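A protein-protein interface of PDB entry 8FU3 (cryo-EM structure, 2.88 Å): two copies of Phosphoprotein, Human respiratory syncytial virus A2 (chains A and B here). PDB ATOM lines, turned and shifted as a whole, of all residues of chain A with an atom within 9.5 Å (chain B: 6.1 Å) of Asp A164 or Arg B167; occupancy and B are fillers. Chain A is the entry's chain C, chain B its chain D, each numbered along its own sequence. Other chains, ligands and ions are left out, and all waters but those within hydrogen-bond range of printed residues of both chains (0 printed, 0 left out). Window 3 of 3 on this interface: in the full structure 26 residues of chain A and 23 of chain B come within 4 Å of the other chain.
Asp A164 touches Arg B167, but with the chains exchanged Arg A167 does not touch Asp B164 (10.8 Å).
Ile B166 touches its own counterpart, Ile A166.
Asp A168 touches Met B170, but with the chains exchanged Met A170 does not touch Asp B168 (11.5 Å).
Ala A169 touches Met B170, but with the chains exchanged Met A170 does not touch Ala B169 (10.6 Å).
Positions printed for both chains: 158, 160, 162, 163, 164, 165, 166, 167, 168, 169 and 170.
Of the 8 pairs that touch across the chains among the printed residues, 1 has its exchanged pair printed and touching as well.
O of Gly A165 touches CG of Arg B167, at 3.98 Å.
Arg B163 touches Ile A166.
Ile A166 touches Ile B166.
Met B170 touches Asp A168 (CE to OD2, 3.7 Å).
Ala A169 touches Ile B166 (CB to CG2, 3.9 Å).
SD of Met B170 touches CB of Ala A169, 3.8 Å away.
Printed residues of chain A within 4 Å of Arg B167: Asp A164 (3.3 Å) and Gly A165 (3.98 Å).
No residue of chain A comes within 4 Å of Gly B165.
No residue of chain A comes within 4 Å of Asp B168.
No residue of chain A comes within 4 Å of Ala B169.
Of the printed residues of chain A, Arg B163 touches Asp A164 (2.6 Å) and Ile A166 (3.6 Å).
Printed residues of chain A within 4 Å of Met B170: Asp A168 (3.7 Å) and Ala A169 (3.8 Å).
The nearest printed residue of chain B that does not touch Ala A169 is Arg B167 (6.5 Å).
Hydrophobic or aromatic side chains of chain B within 4 Å of the printed part of chain A: Ile B166 and Met B170.
Along chain A the printed residues that touch a printed residue of chain B span positions 164 to 169.
Among the printed residues, Asp or Glu carboxylates within 4 Å of a Lys or Arg side-chain nitrogen of the other chain: Asp A164 with Arg B163.
OD1 of Asp B164 lies within salt-bridge range of NH2 of Arg B167, 2.8 Å away.
The backbone carbonyl oxygen of Ser A161 is in hydrogen-bond range of the backbone NH of Ile A166, 2.8 Å away.
NH1 of Arg B163 lies within salt-bridge range of OD2 of Asp A164 (2.6 Å).
The guanidinium group (NH1) of Arg B167 sits at hydrogen-bond distance from the backbone carbonyl oxygen (O) of Asp A164.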
ATOM      1  N   GLY A 158      18.460   0.462  -4.390  1.00  0.00           N
ATOM      2  CA  GLY A 158      18.919   0.801  -3.055  1.00  0.00           C
ATOM      3  C   GLY A 158      20.432   0.907  -2.958  1.00  0.00           C
ATOM      4  O   GLY A 158      21.122   1.005  -3.970  1.00  0.00           O
ATOM      5  N   PRO A 159      20.951   0.844  -1.735  1.00  0.00           N
ATOM      6  CA  PRO A 159      22.339   1.043  -1.359  1.00  0.00           C
ATOM      7  C   PRO A 159      23.254   0.163  -2.164  1.00  0.00           C
ATOM      8  O   PRO A 159      24.381   0.580  -2.498  1.00  0.00           O
ATOM      9  CB  PRO A 159      22.307   0.600   0.113  1.00  0.00           C
ATOM     10  CG  PRO A 159      20.895   0.892   0.554  1.00  0.00           C
ATOM     11  CD  PRO A 159      20.059   0.545  -0.624  1.00  0.00           C
ATOM     12  N   THR A 160      22.807  -1.009  -2.549  1.00  0.00           N
ATOM     13  CA  THR A 160      23.622  -1.900  -3.324  1.00  0.00           C
ATOM     14  C   THR A 160      23.692  -1.478  -4.788  1.00  0.00           C
ATOM     15  O   THR A 160      24.673  -1.753  -5.474  1.00  0.00           O
ATOM     16  CB  THR A 160      23.116  -3.332  -3.230  1.00  0.00           C
ATOM     17  OG1 THR A 160      21.787  -3.387  -3.737  1.00  0.00           O
ATOM     18  CG2 THR A 160      23.121  -3.803  -1.780  1.00  0.00           C
ATOM     19  N   SER A 161      22.655  -0.781  -5.259  1.00  0.00           N
ATOM     20  CA  SER A 161      22.682  -0.323  -6.638  1.00  0.00           C
ATOM     21  C   SER A 161      23.675   0.812  -6.722  1.00  0.00           C
ATOM     22  O   SER A 161      24.379   0.974  -7.725  1.00  0.00           O
ATOM     23  CB  SER A 161      21.316   0.162  -7.069  1.00  0.00           C
ATOM     24  OG  SER A 161      20.994   1.369  -6.452  1.00  0.00           O
ATOM     25  N   ALA A 162      23.779   1.568  -5.641  1.00  0.00           N
ATOM     26  CA  ALA A 162      24.769   2.622  -5.569  1.00  0.00           C
ATOM     27  C   ALA A 162      26.159   2.011  -5.532  1.00  0.00           C
ATOM     28  O   ALA A 162      27.068   2.470  -6.225  1.00  0.00           O
ATOM     29  CB  ALA A 162      24.531   3.506  -4.358  1.00  0.00           C
ATOM     30  N   ARG A 163      26.318   0.944  -4.765  1.00  0.00           N
ATOM     31  CA  ARG A 163      27.609   0.285  -4.624  1.00  0.00           C
ATOM     32  C   ARG A 163      28.177  -0.182  -5.950  1.00  0.00           C
ATOM     33  O   ARG A 163      29.376  -0.039  -6.205  1.00  0.00           O
ATOM     34  CB  ARG A 163      27.511  -0.904  -3.699  1.00  0.00           C
ATOM     35  CG  ARG A 163      28.808  -1.664  -3.504  1.00  0.00           C
ATOM     36  CD  ARG A 163      28.659  -2.728  -2.501  1.00  0.00           C
ATOM     37  NE  ARG A 163      27.665  -3.711  -2.901  1.00  0.00           N
ATOM     38  CZ  ARG A 163      27.025  -4.531  -2.050  1.00  0.00           C
ATOM     39  NH1 ARG A 163      27.287  -4.479  -0.769  1.00  0.00           N
ATOM     40  NH2 ARG A 163      26.129  -5.393  -2.493  1.00  0.00           N
ATOM     41  N   ASP A 164      27.330  -0.742  -6.799  1.00  0.00           N
ATOM     42  CA  ASP A 164      27.796  -1.268  -8.073  1.00  0.00           C
ATOM     43  C   ASP A 164      27.765  -0.238  -9.189  1.00  0.00           C
ATOM     44  O   ASP A 164      28.081  -0.548 -10.338  1.00  0.00           O
ATOM     45  CB  ASP A 164      26.982  -2.493  -8.462  1.00  0.00           C
ATOM     46  CG  ASP A 164      27.302  -3.686  -7.576  1.00  0.00           C
ATOM     47  OD1 ASP A 164      28.419  -3.784  -7.121  1.00  0.00           O
ATOM     48  OD2 ASP A 164      26.434  -4.492  -7.365  1.00  0.00           O
ATOM     49  N   GLY A 165      27.394   0.989  -8.847  1.00  0.00           N
ATOM     50  CA  GLY A 165      27.363   2.072  -9.812  1.00  0.00           C
ATOM     51  C   GLY A 165      26.238   1.944 -10.825  1.00  0.00           C
ATOM     52  O   GLY A 165      26.405   2.338 -11.981  1.00  0.00           O
ATOM     53  N   ILE A 166      25.105   1.376 -10.429  1.00  0.00           N
ATOM     54  CA  ILE A 166      24.015   1.211 -11.377  1.00  0.00           C
ATOM     55  C   ILE A 166      22.737   1.896 -10.925  1.00  0.00           C
ATOM     56  O   ILE A 166      21.677   1.677 -11.512  1.00  0.00           O
ATOM     57  CB  ILE A 166      23.709  -0.267 -11.633  1.00  0.00           C
ATOM     58  CG1 ILE A 166      23.223  -0.930 -10.357  1.00  0.00           C
ATOM     59  CG2 ILE A 166      24.978  -0.958 -12.137  1.00  0.00           C
ATOM     60  CD1 ILE A 166      22.542  -2.249 -10.585  1.00  0.00           C
ATOM     61  N   ARG A 167      22.812   2.699  -9.873  1.00  0.00           N
ATOM     62  CA  ARG A 167      21.598   3.338  -9.388  1.00  0.00           C
ATOM     63  C   ARG A 167      21.043   4.299 -10.419  1.00  0.00           C
ATOM     64  O   ARG A 167      19.831   4.430 -10.572  1.00  0.00           O
ATOM     65  CB  ARG A 167      21.806   4.084  -8.085  1.00  0.00           C
ATOM     66  CG  ARG A 167      20.511   4.637  -7.550  1.00  0.00           C
ATOM     67  CD  ARG A 167      20.585   5.135  -6.182  1.00  0.00           C
ATOM     68  NE  ARG A 167      19.249   5.417  -5.704  1.00  0.00           N
ATOM     69  CZ  ARG A 167      18.575   6.565  -5.920  1.00  0.00           C
ATOM     70  NH1 ARG A 167      19.134   7.553  -6.583  1.00  0.00           N
ATOM     71  NH2 ARG A 167      17.336   6.688  -5.475  1.00  0.00           N
ATOM     72  N   ASP A 168      21.931   4.985 -11.121  1.00  0.00           N
ATOM     73  CA  ASP A 168      21.501   5.956 -12.107  1.00  0.00           C
ATOM     74  C   ASP A 168      20.830   5.245 -13.261  1.00  0.00           C
ATOM     75  O   ASP A 168      19.822   5.703 -13.791  1.00  0.00           O
ATOM     76  CB  ASP A 168      22.701   6.746 -12.610  1.00  0.00           C
ATOM     77  CG  ASP A 168      23.797   5.848 -13.160  1.00  0.00           C
ATOM     78  OD1 ASP A 168      23.731   4.656 -12.938  1.00  0.00           O
ATOM     79  OD2 ASP A 168      24.697   6.355 -13.785  1.00  0.00           O
ATOM     80  N   ALA A 169      21.353   4.082 -13.607  1.00  0.00           N
ATOM     81  CA  ALA A 169      20.763   3.290 -14.667  1.00  0.00           C
ATOM     82  C   ALA A 169      19.343   2.889 -14.308  1.00  0.00           C
ATOM     83  O   ALA A 169      18.446   2.921 -15.147  1.00  0.00           O
ATOM     84  CB  ALA A 169      21.595   2.042 -14.920  1.00  0.00           C
ATOM     85  N   MET A 170      19.134   2.522 -13.052  1.00  0.00           N
ATOM     86  CA  MET A 170      17.819   2.082 -12.622  1.00  0.00           C
ATOM     87  C   MET A 170      16.823   3.223 -12.505  1.00  0.00           C
ATOM     88  O   MET A 170      15.661   3.079 -12.882  1.00  0.00           O
ATOM     89  CB  MET A 170      17.916   1.346 -11.299  1.00  0.00           C
ATOM     90  CG  MET A 170      18.632   0.021 -11.384  1.00  0.00           C
ATOM     91  SD  MET A 170      18.784  -0.792  -9.800  1.00  0.00           S
ATOM     92  CE  MET A 170      17.092  -1.325  -9.508  1.00  0.00           C
ATOM     93  N   GLY B 158      22.521 -10.045 -10.064  1.00  0.00           N
ATOM     94  CA  GLY B 158      23.685  -9.296  -9.604  1.00  0.00           C
ATOM     95  C   GLY B 158      24.961 -10.121  -9.379  1.00  0.00           C
ATOM     96  O   GLY B 158      25.505 -10.121  -8.274  1.00  0.00           O
ATOM     97  N   THR B 160      28.992 -10.368 -10.763  1.00  0.00           N
ATOM     98  CA  THR B 160      29.913  -9.305 -11.112  1.00  0.00           C
ATOM     99  C   THR B 160      29.835  -8.964 -12.592  1.00  0.00           C
ATOM    100  O   THR B 160      29.944  -7.798 -12.972  1.00  0.00           O
ATOM    101  CB  THR B 160      31.358  -9.696 -10.750  1.00  0.00           C
ATOM    102  OG1 THR B 160      31.707 -10.909 -11.434  1.00  0.00           O
ATOM    103  CG2 THR B 160      31.480  -9.911  -9.248  1.00  0.00           C
ATOM    104  N   ALA B 162      27.245  -9.169 -14.755  1.00  0.00           N
ATOM    105  CA  ALA B 162      26.054  -8.422 -15.137  1.00  0.00           C
ATOM    106  C   ALA B 162      26.160  -6.987 -14.674  1.00  0.00           C
ATOM    107  O   ALA B 162      25.831  -6.058 -15.409  1.00  0.00           O
ATOM    108  CB  ALA B 162      24.808  -9.041 -14.539  1.00  0.00           C
ATOM    109  N   ARG B 163      26.630  -6.809 -13.446  1.00  0.00           N
ATOM    110  CA  ARG B 163      26.697  -5.482 -12.868  1.00  0.00           C
ATOM    111  C   ARG B 163      27.761  -4.641 -13.548  1.00  0.00           C
ATOM    112  O   ARG B 163      27.543  -3.457 -13.811  1.00  0.00           O
ATOM    113  CB  ARG B 163      26.934  -5.577 -11.368  1.00  0.00           C
ATOM    114  CG  ARG B 163      25.737  -6.143 -10.584  1.00  0.00           C
ATOM    115  CD  ARG B 163      24.656  -5.127 -10.437  1.00  0.00           C
ATOM    116  NE  ARG B 163      23.416  -5.676  -9.888  1.00  0.00           N
ATOM    117  CZ  ARG B 163      23.133  -5.835  -8.577  1.00  0.00           C
ATOM    118  NH1 ARG B 163      24.004  -5.505  -7.650  1.00  0.00           N
ATOM    119  NH2 ARG B 163      21.960  -6.327  -8.227  1.00  0.00           N
ATOM    120  N   ASP B 164      28.891  -5.254 -13.882  1.00  0.00           N
ATOM    121  CA  ASP B 164      29.924  -4.536 -14.601  1.00  0.00           C
ATOM    122  C   ASP B 164      29.423  -4.203 -15.993  1.00  0.00           C
ATOM    123  O   ASP B 164      29.705  -3.131 -16.522  1.00  0.00           O
ATOM    124  CB  ASP B 164      31.206  -5.359 -14.695  1.00  0.00           C
ATOM    125  CG  ASP B 164      31.961  -5.480 -13.366  1.00  0.00           C
ATOM    126  OD1 ASP B 164      31.649  -4.766 -12.431  1.00  0.00           O
ATOM    127  OD2 ASP B 164      32.861  -6.280 -13.306  1.00  0.00           O
ATOM    128  N   GLY B 165      28.649  -5.114 -16.576  1.00  0.00           N
ATOM    129  CA  GLY B 165      28.086  -4.896 -17.898  1.00  0.00           C
ATOM    130  C   GLY B 165      27.180  -3.673 -17.907  1.00  0.00           C
ATOM    131  O   GLY B 165      27.230  -2.864 -18.835  1.00  0.00           O
ATOM    132  N   ILE B 166      26.367  -3.527 -16.862  1.00  0.00           N
ATOM    133  CA  ILE B 166      25.469  -2.387 -16.765  1.00  0.00           C
ATOM    134  C   ILE B 166      26.258  -1.104 -16.591  1.00  0.00           C
ATOM    135  O   ILE B 166      25.986  -0.106 -17.258  1.00  0.00           O
ATOM    136  CB  ILE B 166      24.502  -2.528 -15.579  1.00  0.00           C
ATOM    137  CG1 ILE B 166      23.557  -3.711 -15.806  1.00  0.00           C
ATOM    138  CG2 ILE B 166      23.709  -1.221 -15.418  1.00  0.00           C
ATOM    139  CD1 ILE B 166      22.811  -4.140 -14.552  1.00  0.00           C
ATOM    140  N   ARG B 167      27.228  -1.124 -15.683  1.00  0.00           N
ATOM    141  CA  ARG B 167      28.023   0.063 -15.411  1.00  0.00           C
ATOM    142  C   ARG B 167      28.805   0.489 -16.647  1.00  0.00           C
ATOM    143  O   ARG B 167      28.845   1.674 -16.982  1.00  0.00           O
ATOM    144  CB  ARG B 167      28.973  -0.184 -14.255  1.00  0.00           C
ATOM    145  CG  ARG B 167      29.725   1.049 -13.763  1.00  0.00           C
ATOM    146  CD  ARG B 167      30.521   0.756 -12.546  1.00  0.00           C
ATOM    147  NE  ARG B 167      31.601  -0.172 -12.826  1.00  0.00           N
ATOM    148  CZ  ARG B 167      31.631  -1.478 -12.472  1.00  0.00           C
ATOM    149  NH1 ARG B 167      30.635  -2.040 -11.811  1.00  0.00           N
ATOM    150  NH2 ARG B 167      32.671  -2.218 -12.801  1.00  0.00           N
ATOM    151  N   ASP B 168      29.415  -0.474 -17.332  1.00  0.00           N
ATOM    152  CA  ASP B 168      30.187  -0.164 -18.524  1.00  0.00           C
ATOM    153  C   ASP B 168      29.280   0.364 -19.618  1.00  0.00           C
ATOM    154  O   ASP B 168      29.667   1.253 -20.381  1.00  0.00           O
ATOM    155  CB  ASP B 168      30.944  -1.394 -19.020  1.00  0.00           C
ATOM    156  CG  ASP B 168      32.122  -1.783 -18.123  1.00  0.00           C
ATOM    157  OD1 ASP B 168      32.507  -1.001 -17.283  1.00  0.00           O
ATOM    158  OD2 ASP B 168      32.634  -2.861 -18.301  1.00  0.00           O
ATOM    159  N   ALA B 169      28.065  -0.173 -19.691  1.00  0.00           N
ATOM    160  CA  ALA B 169      27.097   0.299 -20.665  1.00  0.00           C
ATOM    161  C   ALA B 169      26.756   1.757 -20.394  1.00  0.00           C
ATOM    162  O   ALA B 169      26.596   2.546 -21.326  1.00  0.00           O
ATOM    163  CB  ALA B 169      25.844  -0.553 -20.626  1.00  0.00           C
ATOM    164  N   MET B 170      26.670   2.119 -19.115  1.00  0.00           N
ATOM    165  CA  MET B 170      26.383   3.495 -18.730  1.00  0.00           C
ATOM    166  C   MET B 170      27.543   4.423 -19.064  1.00  0.00           C
ATOM    167  O   MET B 170      27.333   5.590 -19.399  1.00  0.00           O
ATOM    168  CB  MET B 170      26.043   3.576 -17.248  1.00  0.00           C
ATOM    169  CG  MET B 170      24.703   2.988 -16.890  1.00  0.00           C
ATOM    170  SD  MET B 170      23.349   3.739 -17.806  1.00  0.00           S
ATOM    171  CE  MET B 170      23.278   5.378 -17.079  1.00  0.00           C
ATOM    172  N   ILE B 171      28.765   3.902 -19.010  1.00  0.00           N
ATOM    173  CA  ILE B 171      29.917   4.695 -19.412  1.00  0.00           C
ATOM    174  C   ILE B 171      29.810   4.970 -20.898  1.00  0.00           C
ATOM    175  O   ILE B 171      29.987   6.104 -21.345  1.00  0.00           O
ATOM    176  CB  ILE B 171      31.248   3.984 -19.101  1.00  0.00           C
ATOM    177  CG1 ILE B 171      31.438   3.890 -17.578  1.00  0.00           C
ATOM    178  CG2 ILE B 171      32.411   4.738 -19.760  1.00  0.00           C
ATOM    179  CD1 ILE B 171      32.562   2.963 -17.141  1.00  0.00           C
ATOM    180  N   GLY B 172      29.494   3.926 -21.656  1.00  0.00           N
ATOM    181  CA  GLY B 172      29.298   4.060 -23.088  1.00  0.00           C
ATOM    182  C   GLY B 172      28.138   5.002 -23.379  1.00  0.00           C
ATOM    183  O   GLY B 172      28.195   5.781 -24.330  1.00  0.00           O
